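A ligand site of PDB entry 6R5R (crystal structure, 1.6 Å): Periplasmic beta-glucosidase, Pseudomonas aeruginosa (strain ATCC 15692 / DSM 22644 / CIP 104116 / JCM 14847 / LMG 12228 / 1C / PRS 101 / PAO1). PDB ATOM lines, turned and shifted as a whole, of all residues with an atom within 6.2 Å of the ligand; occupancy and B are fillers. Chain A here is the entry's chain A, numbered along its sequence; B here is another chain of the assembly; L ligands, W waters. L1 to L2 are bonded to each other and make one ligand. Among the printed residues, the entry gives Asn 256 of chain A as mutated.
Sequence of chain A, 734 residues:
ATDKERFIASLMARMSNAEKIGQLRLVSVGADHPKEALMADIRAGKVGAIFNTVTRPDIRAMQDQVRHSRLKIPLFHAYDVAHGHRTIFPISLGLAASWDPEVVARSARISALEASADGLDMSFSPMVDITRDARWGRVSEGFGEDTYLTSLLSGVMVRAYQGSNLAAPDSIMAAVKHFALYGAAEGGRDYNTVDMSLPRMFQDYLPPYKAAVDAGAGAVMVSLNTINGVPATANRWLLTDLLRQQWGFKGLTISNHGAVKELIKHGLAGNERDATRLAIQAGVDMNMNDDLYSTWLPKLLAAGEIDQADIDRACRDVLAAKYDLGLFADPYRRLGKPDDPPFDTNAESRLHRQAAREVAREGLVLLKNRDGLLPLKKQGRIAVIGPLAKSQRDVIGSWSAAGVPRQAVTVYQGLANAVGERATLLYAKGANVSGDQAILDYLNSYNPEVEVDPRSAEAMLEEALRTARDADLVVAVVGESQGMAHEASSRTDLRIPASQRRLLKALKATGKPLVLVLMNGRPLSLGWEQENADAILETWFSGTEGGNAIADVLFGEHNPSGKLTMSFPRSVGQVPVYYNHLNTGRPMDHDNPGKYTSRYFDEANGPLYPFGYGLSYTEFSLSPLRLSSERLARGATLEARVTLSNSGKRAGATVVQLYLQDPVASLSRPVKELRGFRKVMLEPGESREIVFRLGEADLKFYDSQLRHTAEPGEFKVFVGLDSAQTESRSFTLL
The side-chain carboxylate (OD1) of Asp 80 is in hydrogen-bond range of an oxygen (O2) of LIG L1. NE2 of His 178 lies within hydrogen-bond range of O1 of LIG L1 (2.7 Å). An oxygen (O6) of LIG L1 sits at hydrogen-bond distance from the side-chain carboxylate (OE2) of Glu 487, at 2.7 Å. O1 of LIG L1 sits at hydrogen-bond distance from NZ of Lys 177, at 2.8 Å. O2 of LG2 L2 lies within hydrogen-bond range of ND2 of Asn 52, 2.9 Å away. O1 of LIG L1 lies within hydrogen-bond range of NH2 of Arg 138, 2.9 Å away. The side-chain sulfur (SD) of Met 221 is in hydrogen-bond range of an oxygen (O2) of LIG L1 (3.5 Å).
Merely in contact with the ligand: Phe 51, His 257, Asn 256, Phe 124, Leu 224, Met 288, Tyr 595 of chain B and Trp 399. Hydrophobic or aromatic side chains that line the ligand: Phe 51, Phe 124, His 178, Met 221, Leu 224, His 257, Met 288, Trp 399 and Tyr 595 of chain B. Of the 21 residues printed, 15 come within 4 Å of the ligand. The nearest printed residue that does not touch the ligand is Arg 585 of chain B (4.1 Å).
OD1 of Asp 80 is in salt-bridge range of NZ of Lys 177 (3.2 Å). The guanidinium group (NH1) of Arg 585 of chain B lies within salt-bridge range of the side-chain carboxylate (OE2) of Glu 487 (3.1 Å). The side-chain carboxylate (OE2) of Glu 487 is in hydrogen-bond range of the side-chain hydroxyl (OH) of Tyr 191, at 2.6 Å. O of Phe 124 is in hydrogen-bond range of NZ of Lys 177, 2.8 Å away. The guanidinium group of Arg 138 lies within hydrogen-bond range of the side-chain hydroxyl of Tyr 182 (3.0 Å). The side-chain sulfur of Met 288 lies within hydrogen-bond range of the backbone NH of His 257 (3.7 Å). O of Tyr 79 is in hydrogen-bond range of N of Phe 124, 2.9 Å away. The indole nitrogen (NE1) of Trp 399 is in hydrogen-bond range of the side-chain carboxylate (OE2) of Glu 141 (2.9 Å).
Water W3 lies within hydrogen-bond range of an oxygen (O5) of LG2 L2 (2.8 Å) and the guanidinium group of Arg 585 of chain B (2.9 Å). Water W1 lies within hydrogen-bond range of OD2 of Asp 80 (2.7 Å), O2 of LG2 L2 (2.8 Å) and OD1 of Asn 52 (3.0 Å). Water W2 lies within hydrogen-bond range of the side-chain amide nitrogen (ND2) of Asn 256 (2.8 Å), an oxygen (O6) of LIG L1 (2.9 Å), the guanidinium group (NH1) of Arg 138 (3.3 Å) and a ring nitrogen (NE2) of His 178 (3.3 Å).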
ATOM      1  N   PHE A  51      26.166   9.970  36.932  1.00  0.00           N
ATOM      2  CA  PHE A  51      25.049  10.830  36.504  1.00  0.00           C
ATOM      3  C   PHE A  51      23.798  10.515  37.319  1.00  0.00           C
ATOM      4  O   PHE A  51      23.665   9.404  37.881  1.00  0.00           O
ATOM      5  CB  PHE A  51      24.830  10.753  34.990  1.00  0.00           C
ATOM      6  CG  PHE A  51      24.286   9.441  34.476  1.00  0.00           C
ATOM      7  CD1 PHE A  51      25.125   8.355  34.333  1.00  0.00           C
ATOM      8  CD2 PHE A  51      22.960   9.301  34.121  1.00  0.00           C
ATOM      9  CE1 PHE A  51      24.661   7.148  33.830  1.00  0.00           C
ATOM     10  CE2 PHE A  51      22.491   8.076  33.665  1.00  0.00           C
ATOM     11  CZ  PHE A  51      23.336   7.006  33.535  1.00  0.00           C
ATOM     12  N   ASN A  52      22.896  11.519  37.399  1.00  0.00           N
ATOM     13  CA  ASN A  52      21.572  11.414  38.055  1.00  0.00           C
ATOM     14  C   ASN A  52      21.656  11.339  39.597  1.00  0.00           C
ATOM     15  O   ASN A  52      20.566  11.145  40.186  1.00  0.00           O
ATOM     16  CB  ASN A  52      20.779  10.237  37.523  1.00  0.00           C
ATOM     17  CG  ASN A  52      20.202  10.461  36.151  1.00  0.00           C
ATOM     18  OD1 ASN A  52      20.236  11.578  35.661  1.00  0.00           O
ATOM     19  ND2 ASN A  52      19.720   9.393  35.547  1.00  0.00           N
ATOM     20  N   TYR A  79      24.349  15.696  35.151  1.00  0.00           N
ATOM     21  CA  TYR A  79      22.891  15.655  35.117  1.00  0.00           C
ATOM     22  C   TYR A  79      22.380  16.297  33.823  1.00  0.00           C
ATOM     23  O   TYR A  79      23.110  16.991  33.160  1.00  0.00           O
ATOM     24  CB  TYR A  79      22.295  16.333  36.345  1.00  0.00           C
ATOM     25  CG  TYR A  79      20.854  16.084  36.665  1.00  0.00           C
ATOM     26  CD1 TYR A  79      20.261  14.837  36.540  1.00  0.00           C
ATOM     27  CD2 TYR A  79      20.074  17.126  37.161  1.00  0.00           C
ATOM     28  CE1 TYR A  79      18.942  14.604  36.875  1.00  0.00           C
ATOM     29  CE2 TYR A  79      18.748  16.906  37.514  1.00  0.00           C
ATOM     30  CZ  TYR A  79      18.190  15.654  37.349  1.00  0.00           C
ATOM     31  OH  TYR A  79      16.898  15.372  37.697  1.00  0.00           O
ATOM     32  N   ASP A  80      21.105  16.059  33.568  1.00  0.00           N
ATOM     33  CA  ASP A  80      20.384  16.610  32.392  1.00  0.00           C
ATOM     34  C   ASP A  80      19.763  17.946  32.789  1.00  0.00           C
ATOM     35  O   ASP A  80      18.559  18.027  32.998  1.00  0.00           O
ATOM     36  CB  ASP A  80      19.383  15.589  31.881  1.00  0.00           C
ATOM     37  CG  ASP A  80      20.064  14.477  31.092  1.00  0.00           C
ATOM     38  OD1 ASP A  80      20.755  14.797  30.090  1.00  0.00           O
ATOM     39  OD2 ASP A  80      19.906  13.280  31.512  1.00  0.00           O
ATOM     40  N   PHE A 124      24.572  17.575  30.682  1.00  0.00           N
ATOM     41  CA  PHE A 124      24.414  17.074  29.305  1.00  0.00           C
ATOM     42  C   PHE A 124      23.528  18.071  28.572  1.00  0.00           C
ATOM     43  O   PHE A 124      22.321  17.860  28.396  1.00  0.00           O
ATOM     44  CB  PHE A 124      23.797  15.689  29.343  1.00  0.00           C
ATOM     45  CG  PHE A 124      24.592  14.659  30.098  1.00  0.00           C
ATOM     46  CD1 PHE A 124      25.958  14.527  29.973  1.00  0.00           C
ATOM     47  CD2 PHE A 124      23.921  13.801  30.959  1.00  0.00           C
ATOM     48  CE1 PHE A 124      26.623  13.545  30.703  1.00  0.00           C
ATOM     49  CE2 PHE A 124      24.597  12.846  31.686  1.00  0.00           C
ATOM     50  CZ  PHE A 124      25.944  12.708  31.525  1.00  0.00           C
ATOM     51  N   ARG A 138      11.540  15.324  20.526  1.00  0.00           N
ATOM     52  CA  ARG A 138      12.685  16.055  21.117  1.00  0.00           C
ATOM     53  C   ARG A 138      12.857  17.433  20.498  1.00  0.00           C
ATOM     54  O   ARG A 138      13.850  18.111  20.827  1.00  0.00           O
ATOM     55  CB  ARG A 138      13.937  15.193  21.063  1.00  0.00           C
ATOM     56  CG  ARG A 138      13.683  13.867  21.765  1.00  0.00           C
ATOM     57  CD  ARG A 138      14.958  13.095  22.042  1.00  0.00           C
ATOM     58  NE  ARG A 138      15.674  13.695  23.175  1.00  0.00           N
ATOM     59  CZ  ARG A 138      16.525  13.055  23.973  1.00  0.00           C
ATOM     60  NH1 ARG A 138      16.856  11.788  23.774  1.00  0.00           N
ATOM     61  NH2 ARG A 138      17.025  13.777  24.964  1.00  0.00           N
ATOM     62  N   GLU A 141      13.598  20.325  22.838  1.00  0.00           N
ATOM     63  CA  GLU A 141      14.913  20.481  23.501  1.00  0.00           C
ATOM     64  C   GLU A 141      15.887  21.321  22.680  1.00  0.00           C
ATOM     65  O   GLU A 141      16.892  21.718  23.225  1.00  0.00           O
ATOM     66  CB  GLU A 141      15.558  19.142  23.710  1.00  0.00           C
ATOM     67  CG  GLU A 141      14.762  18.276  24.598  1.00  0.00           C
ATOM     68  CD  GLU A 141      15.222  16.845  24.520  1.00  0.00           C
ATOM     69  OE1 GLU A 141      16.460  16.572  24.645  1.00  0.00           O
ATOM     70  OE2 GLU A 141      14.311  16.023  24.324  1.00  0.00           O
ATOM     71  N   LYS A 177      25.214  18.138  22.960  1.00  0.00           N
ATOM     72  CA  LYS A 177      24.577  16.894  22.436  1.00  0.00           C
ATOM     73  C   LYS A 177      23.632  17.288  21.304  1.00  0.00           C
ATOM     74  O   LYS A 177      23.247  18.436  21.168  1.00  0.00           O
ATOM     75  CB  LYS A 177      23.895  16.204  23.605  1.00  0.00           C
ATOM     76  CG  LYS A 177      22.611  16.857  24.096  1.00  0.00           C
ATOM     77  CD  LYS A 177      22.155  16.262  25.405  1.00  0.00           C
ATOM     78  CE  LYS A 177      20.806  16.719  25.905  1.00  0.00           C
ATOM     79  NZ  LYS A 177      20.550  16.081  27.216  1.00  0.00           N
ATOM     80  N   HIS A 178      23.202  16.351  20.480  1.00  0.00           N
ATOM     81  CA  HIS A 178      23.600  14.951  20.427  1.00  0.00           C
ATOM     82  C   HIS A 178      24.431  14.812  19.152  1.00  0.00           C
ATOM     83  O   HIS A 178      23.883  14.936  18.037  1.00  0.00           O
ATOM     84  CB  HIS A 178      22.411  14.053  20.397  1.00  0.00           C
ATOM     85  CG  HIS A 178      21.470  14.191  21.534  1.00  0.00           C
ATOM     86  ND1 HIS A 178      20.441  15.091  21.525  1.00  0.00           N
ATOM     87  CD2 HIS A 178      21.374  13.523  22.717  1.00  0.00           C
ATOM     88  CE1 HIS A 178      19.768  14.977  22.684  1.00  0.00           C
ATOM     89  NE2 HIS A 178      20.302  14.014  23.395  1.00  0.00           N
ATOM     90  N   TYR A 182      20.819  13.983  15.095  1.00  0.00           N
ATOM     91  CA  TYR A 182      19.811  13.165  15.768  1.00  0.00           C
ATOM     92  C   TYR A 182      18.401  13.644  15.398  1.00  0.00           C
ATOM     93  O   TYR A 182      17.511  12.834  15.267  1.00  0.00           O
ATOM     94  CB  TYR A 182      20.098  13.278  17.267  1.00  0.00           C
ATOM     95  CG  TYR A 182      19.237  12.502  18.219  1.00  0.00           C
ATOM     96  CD1 TYR A 182      18.769  11.220  17.976  1.00  0.00           C
ATOM     97  CD2 TYR A 182      18.947  13.088  19.451  1.00  0.00           C
ATOM     98  CE1 TYR A 182      17.954  10.569  18.914  1.00  0.00           C
ATOM     99  CE2 TYR A 182      18.156  12.448  20.380  1.00  0.00           C
ATOM    100  CZ  TYR A 182      17.642  11.194  20.115  1.00  0.00           C
ATOM    101  OH  TYR A 182      16.826  10.587  21.057  1.00  0.00           O
ATOM    102  N   ASP A 190      11.725   8.657  17.046  1.00  0.00           N
ATOM    103  CA  ASP A 190      12.958   8.843  17.826  1.00  0.00           C
ATOM    104  C   ASP A 190      13.909   7.676  17.542  1.00  0.00           C
ATOM    105  O   ASP A 190      13.477   6.541  17.285  1.00  0.00           O
ATOM    106  CB  ASP A 190      12.653   9.002  19.293  1.00  0.00           C
ATOM    107  CG  ASP A 190      13.731   9.823  20.046  1.00  0.00           C
ATOM    108  OD1 ASP A 190      14.809  10.125  19.489  1.00  0.00           O
ATOM    109  OD2 ASP A 190      13.499  10.085  21.269  1.00  0.00           O
ATOM    110  N   TYR A 191      15.202   7.999  17.559  1.00  0.00           N
ATOM    111  CA  TYR A 191      16.310   7.051  17.399  1.00  0.00           C
ATOM    112  C   TYR A 191      16.438   6.540  15.962  1.00  0.00           C
ATOM    113  O   TYR A 191      17.350   5.734  15.694  1.00  0.00           O
ATOM    114  CB  TYR A 191      16.145   5.835  18.304  1.00  0.00           C
ATOM    115  CG  TYR A 191      15.628   6.098  19.681  1.00  0.00           C
ATOM    116  CD1 TYR A 191      16.293   6.922  20.559  1.00  0.00           C
ATOM    117  CD2 TYR A 191      14.447   5.529  20.113  1.00  0.00           C
ATOM    118  CE1 TYR A 191      15.847   7.119  21.853  1.00  0.00           C
ATOM    119  CE2 TYR A 191      13.994   5.696  21.396  1.00  0.00           C
ATOM    120  CZ  TYR A 191      14.664   6.531  22.258  1.00  0.00           C
ATOM    121  OH  TYR A 191      14.245   6.642  23.567  1.00  0.00           O
ATOM    122  N   MET A 221      28.460  14.728  23.952  1.00  0.00           N
ATOM    123  CA  MET A 221      27.654  13.489  24.074  1.00  0.00           C
ATOM    124  C   MET A 221      27.267  12.980  22.689  1.00  0.00           C
ATOM    125  O   MET A 221      26.697  13.727  21.870  1.00  0.00           O
ATOM    126  CB  MET A 221      26.397  13.676  24.899  1.00  0.00           C
ATOM    127  CG  MET A 221      25.665  12.404  25.023  1.00  0.00           C
ATOM    128  SD  MET A 221      24.163  12.532  26.038  1.00  0.00           S
ATOM    129  CE  MET A 221      24.829  12.091  27.645  1.00  0.00           C
ATOM    130  N   LEU A 224      22.476   8.589  19.396  1.00  0.00           N
ATOM    131  CA  LEU A 224      21.988   7.189  19.305  1.00  0.00           C
ATOM    132  C   LEU A 224      21.710   6.751  17.879  1.00  0.00           C
ATOM    133  O   LEU A 224      21.506   5.545  17.665  1.00  0.00           O
ATOM    134  CB  LEU A 224      20.692   7.110  20.126  1.00  0.00           C
ATOM    135  CG  LEU A 224      20.869   7.167  21.638  1.00  0.00           C
ATOM    136  CD1 LEU A 224      19.525   7.437  22.313  1.00  0.00           C
ATOM    137  CD2 LEU A 224      21.515   5.901  22.122  1.00  0.00           C
ATOM    138  N   ASN A 256      26.156   7.767  24.671  1.00  0.00           N
ATOM    139  CA  ASN A 256      24.793   7.903  25.188  1.00  0.00           C
ATOM    140  C   ASN A 256      24.470   6.649  26.001  1.00  0.00           C
ATOM    141  O   ASN A 256      25.282   5.692  26.148  1.00  0.00           O
ATOM    142  CB  ASN A 256      23.858   8.132  23.998  1.00  0.00           C
ATOM    143  CG  ASN A 256      22.768   9.099  24.290  1.00  0.00           C
ATOM    144  OD1 ASN A 256      22.093   8.890  25.271  1.00  0.00           O
ATOM    145  ND2 ASN A 256      22.612  10.143  23.460  1.00  0.00           N
ATOM    146  N   HIS A 257      23.269   6.592  26.481  1.00  0.00           N
ATOM    147  CA  HIS A 257      22.870   5.663  27.537  1.00  0.00           C
ATOM    148  C   HIS A 257      22.674   4.250  26.998  1.00  0.00           C
ATOM    149  O   HIS A 257      21.795   4.052  26.205  1.00  0.00           O
ATOM    150  CB  HIS A 257      21.591   6.239  28.139  1.00  0.00           C
ATOM    151  CG  HIS A 257      21.226   5.497  29.369  1.00  0.00           C
ATOM    152  ND1 HIS A 257      20.685   4.222  29.307  1.00  0.00           N
ATOM    153  CD2 HIS A 257      21.290   5.874  30.682  1.00  0.00           C
ATOM    154  CE1 HIS A 257      20.481   3.799  30.555  1.00  0.00           C
ATOM    155  NE2 HIS A 257      20.800   4.818  31.421  1.00  0.00           N
ATOM    156  N   MET A 288      28.621   5.056  29.030  1.00  0.00           N
ATOM    157  CA  MET A 288      27.454   5.333  29.896  1.00  0.00           C
ATOM    158  C   MET A 288      26.620   4.077  30.134  1.00  0.00           C
ATOM    159  O   MET A 288      26.073   3.512  29.182  1.00  0.00           O
ATOM    160  CB  MET A 288      26.623   6.480  29.307  1.00  0.00           C
ATOM    161  CG  MET A 288      25.498   6.920  30.171  1.00  0.00           C
ATOM    162  SD  MET A 288      24.772   8.447  29.360  1.00  0.00           S
ATOM    163  CE  MET A 288      23.941   9.248  30.716  1.00  0.00           C
ATOM    164  N   TRP A 399      12.165  17.056  30.329  1.00  0.00           N
ATOM    165  CA  TRP A 399      13.563  17.284  30.781  1.00  0.00           C
ATOM    166  C   TRP A 399      13.618  18.417  31.797  1.00  0.00           C
ATOM    167  O   TRP A 399      14.371  19.394  31.619  1.00  0.00           O
ATOM    168  CB  TRP A 399      14.534  17.478  29.614  1.00  0.00           C
ATOM    169  CG  TRP A 399      14.686  16.229  28.766  1.00  0.00           C
ATOM    170  CD1 TRP A 399      14.182  16.086  27.499  1.00  0.00           C
ATOM    171  CD2 TRP A 399      15.313  14.959  29.091  1.00  0.00           C
ATOM    172  NE1 TRP A 399      14.463  14.826  27.012  1.00  0.00           N
ATOM    173  CE2 TRP A 399      15.157  14.120  27.963  1.00  0.00           C
ATOM    174  CE3 TRP A 399      16.025  14.460  30.198  1.00  0.00           C
ATOM    175  CZ2 TRP A 399      15.619  12.802  27.936  1.00  0.00           C
ATOM    176  CZ3 TRP A 399      16.488  13.155  30.169  1.00  0.00           C
ATOM    177  CH2 TRP A 399      16.298  12.341  29.046  1.00  0.00           C
ATOM    178  N   GLU A 487      11.323  12.498  24.937  1.00  0.00           N
ATOM    179  CA  GLU A 487      12.034  11.381  24.305  1.00  0.00           C
ATOM    180  C   GLU A 487      11.034  10.276  23.975  1.00  0.00           C
ATOM    181  O   GLU A 487      10.223   9.897  24.834  1.00  0.00           O
ATOM    182  CB  GLU A 487      13.091  10.850  25.270  1.00  0.00           C
ATOM    183  CG  GLU A 487      13.885   9.728  24.675  1.00  0.00           C
ATOM    184  CD  GLU A 487      14.882   9.078  25.603  1.00  0.00           C
ATOM    185  OE1 GLU A 487      14.975   9.537  26.768  1.00  0.00           O
ATOM    186  OE2 GLU A 487      15.599   8.140  25.167  1.00  0.00           O
ATOM    187  N   ARG B 585      17.150   0.912  19.110  1.00  0.00           N
ATOM    188  CA  ARG B 585      15.965   0.740  20.006  1.00  0.00           C
ATOM    189  C   ARG B 585      14.765   0.388  19.138  1.00  0.00           C
ATOM    190  O   ARG B 585      13.800   1.155  19.037  1.00  0.00           O
ATOM    191  CB  ARG B 585      15.726   2.026  20.800  1.00  0.00           C
ATOM    192  CG  ARG B 585      16.860   2.339  21.769  1.00  0.00           C
ATOM    193  CD  ARG B 585      16.691   3.587  22.574  1.00  0.00           C
ATOM    194  NE  ARG B 585      17.849   3.791  23.416  1.00  0.00           N
ATOM    195  CZ  ARG B 585      17.858   4.576  24.483  1.00  0.00           C
ATOM    196  NH1 ARG B 585      16.749   5.232  24.834  1.00  0.00           N
ATOM    197  NH2 ARG B 585      18.977   4.711  25.190  1.00  0.00           N
ATOM    198  N   TYR B 595      10.462   3.192  25.199  1.00  0.00           N
ATOM    199  CA  TYR B 595      11.730   3.826  24.728  1.00  0.00           C
ATOM    200  C   TYR B 595      12.242   3.095  23.499  1.00  0.00           C
ATOM    201  O   TYR B 595      13.356   2.514  23.499  1.00  0.00           O
ATOM    202  CB  TYR B 595      12.732   3.959  25.870  1.00  0.00           C
ATOM    203  CG  TYR B 595      12.263   4.988  26.876  1.00  0.00           C
ATOM    204  CD1 TYR B 595      12.409   6.341  26.607  1.00  0.00           C
ATOM    205  CD2 TYR B 595      11.604   4.619  28.031  1.00  0.00           C
ATOM    206  CE1 TYR B 595      11.941   7.313  27.487  1.00  0.00           C
ATOM    207  CE2 TYR B 595      11.125   5.577  28.911  1.00  0.00           C
ATOM    208  CZ  TYR B 595      11.302   6.922  28.647  1.00  0.00           C
ATOM    209  OH  TYR B 595      10.862   7.889  29.508  1.00  0.00           O
HETATM  210  C1  LIG L   1      20.451  12.467  27.975  1.00  0.00           C
HETATM  211  C2  LIG L   1      20.789  11.111  28.619  1.00  0.00           C
HETATM  212  C3  LIG L   1      19.557  10.250  28.374  1.00  0.00           C
HETATM  213  C4  LIG L   1      19.324  10.104  26.872  1.00  0.00           C
HETATM  214  C5  LIG L   1      18.189   9.166  26.471  1.00  0.00           C
HETATM  215  C6  LIG L   1      20.071  12.344  26.500  1.00  0.00           C
HETATM  216  O1  LIG L   1      19.741  13.640  26.019  1.00  0.00           O
HETATM  217  O2  LIG L   1      21.512  13.429  28.129  1.00  0.00           O
HETATM  218  O3  LIG L   1      20.958  11.314  30.063  1.00  0.00           O
HETATM  219  O4  LIG L   1      19.786   8.986  28.905  1.00  0.00           O
HETATM  220  O5  LIG L   1      18.995  11.407  26.358  1.00  0.00           O
HETATM  221  O6  LIG L   1      18.082   9.285  25.026  1.00  0.00           O
HETATM  222  C1  LG2 L   2      18.887   9.398  31.203  1.00  0.00           C
HETATM  223  C2  LG2 L   2      17.957   8.759  32.198  1.00  0.00           C
HETATM  224  C3  LG2 L   2      16.583   8.598  31.524  1.00  0.00           C
HETATM  225  C4  LG2 L   2      16.695   7.851  30.198  1.00  0.00           C
HETATM  226  C5  LG2 L   2      15.332   7.803  29.517  1.00  0.00           C
HETATM  227  C6  LG2 L   2      18.872   8.550  29.942  1.00  0.00           C
HETATM  228  O1  LG2 L   2      20.197   9.414  31.821  1.00  0.00           O
HETATM  229  O2  LG2 L   2      17.905   9.668  33.315  1.00  0.00           O
HETATM  230  O3  LG2 L   2      15.770   7.838  32.427  1.00  0.00           O
HETATM  231  O4  LG2 L   2      17.604   8.532  29.324  1.00  0.00           O
HETATM  232  O5  LG2 L   2      15.604   7.224  28.245  1.00  0.00           O
HETATM  233  O   HOH W   1      18.354  12.399  33.522  1.00  0.00           O
HETATM  234  O   HOH W   2      19.919  10.753  23.344  1.00  0.00           O
HETATM  235  O   HOH W   3      17.895   5.805  27.670  1.00  0.00           O
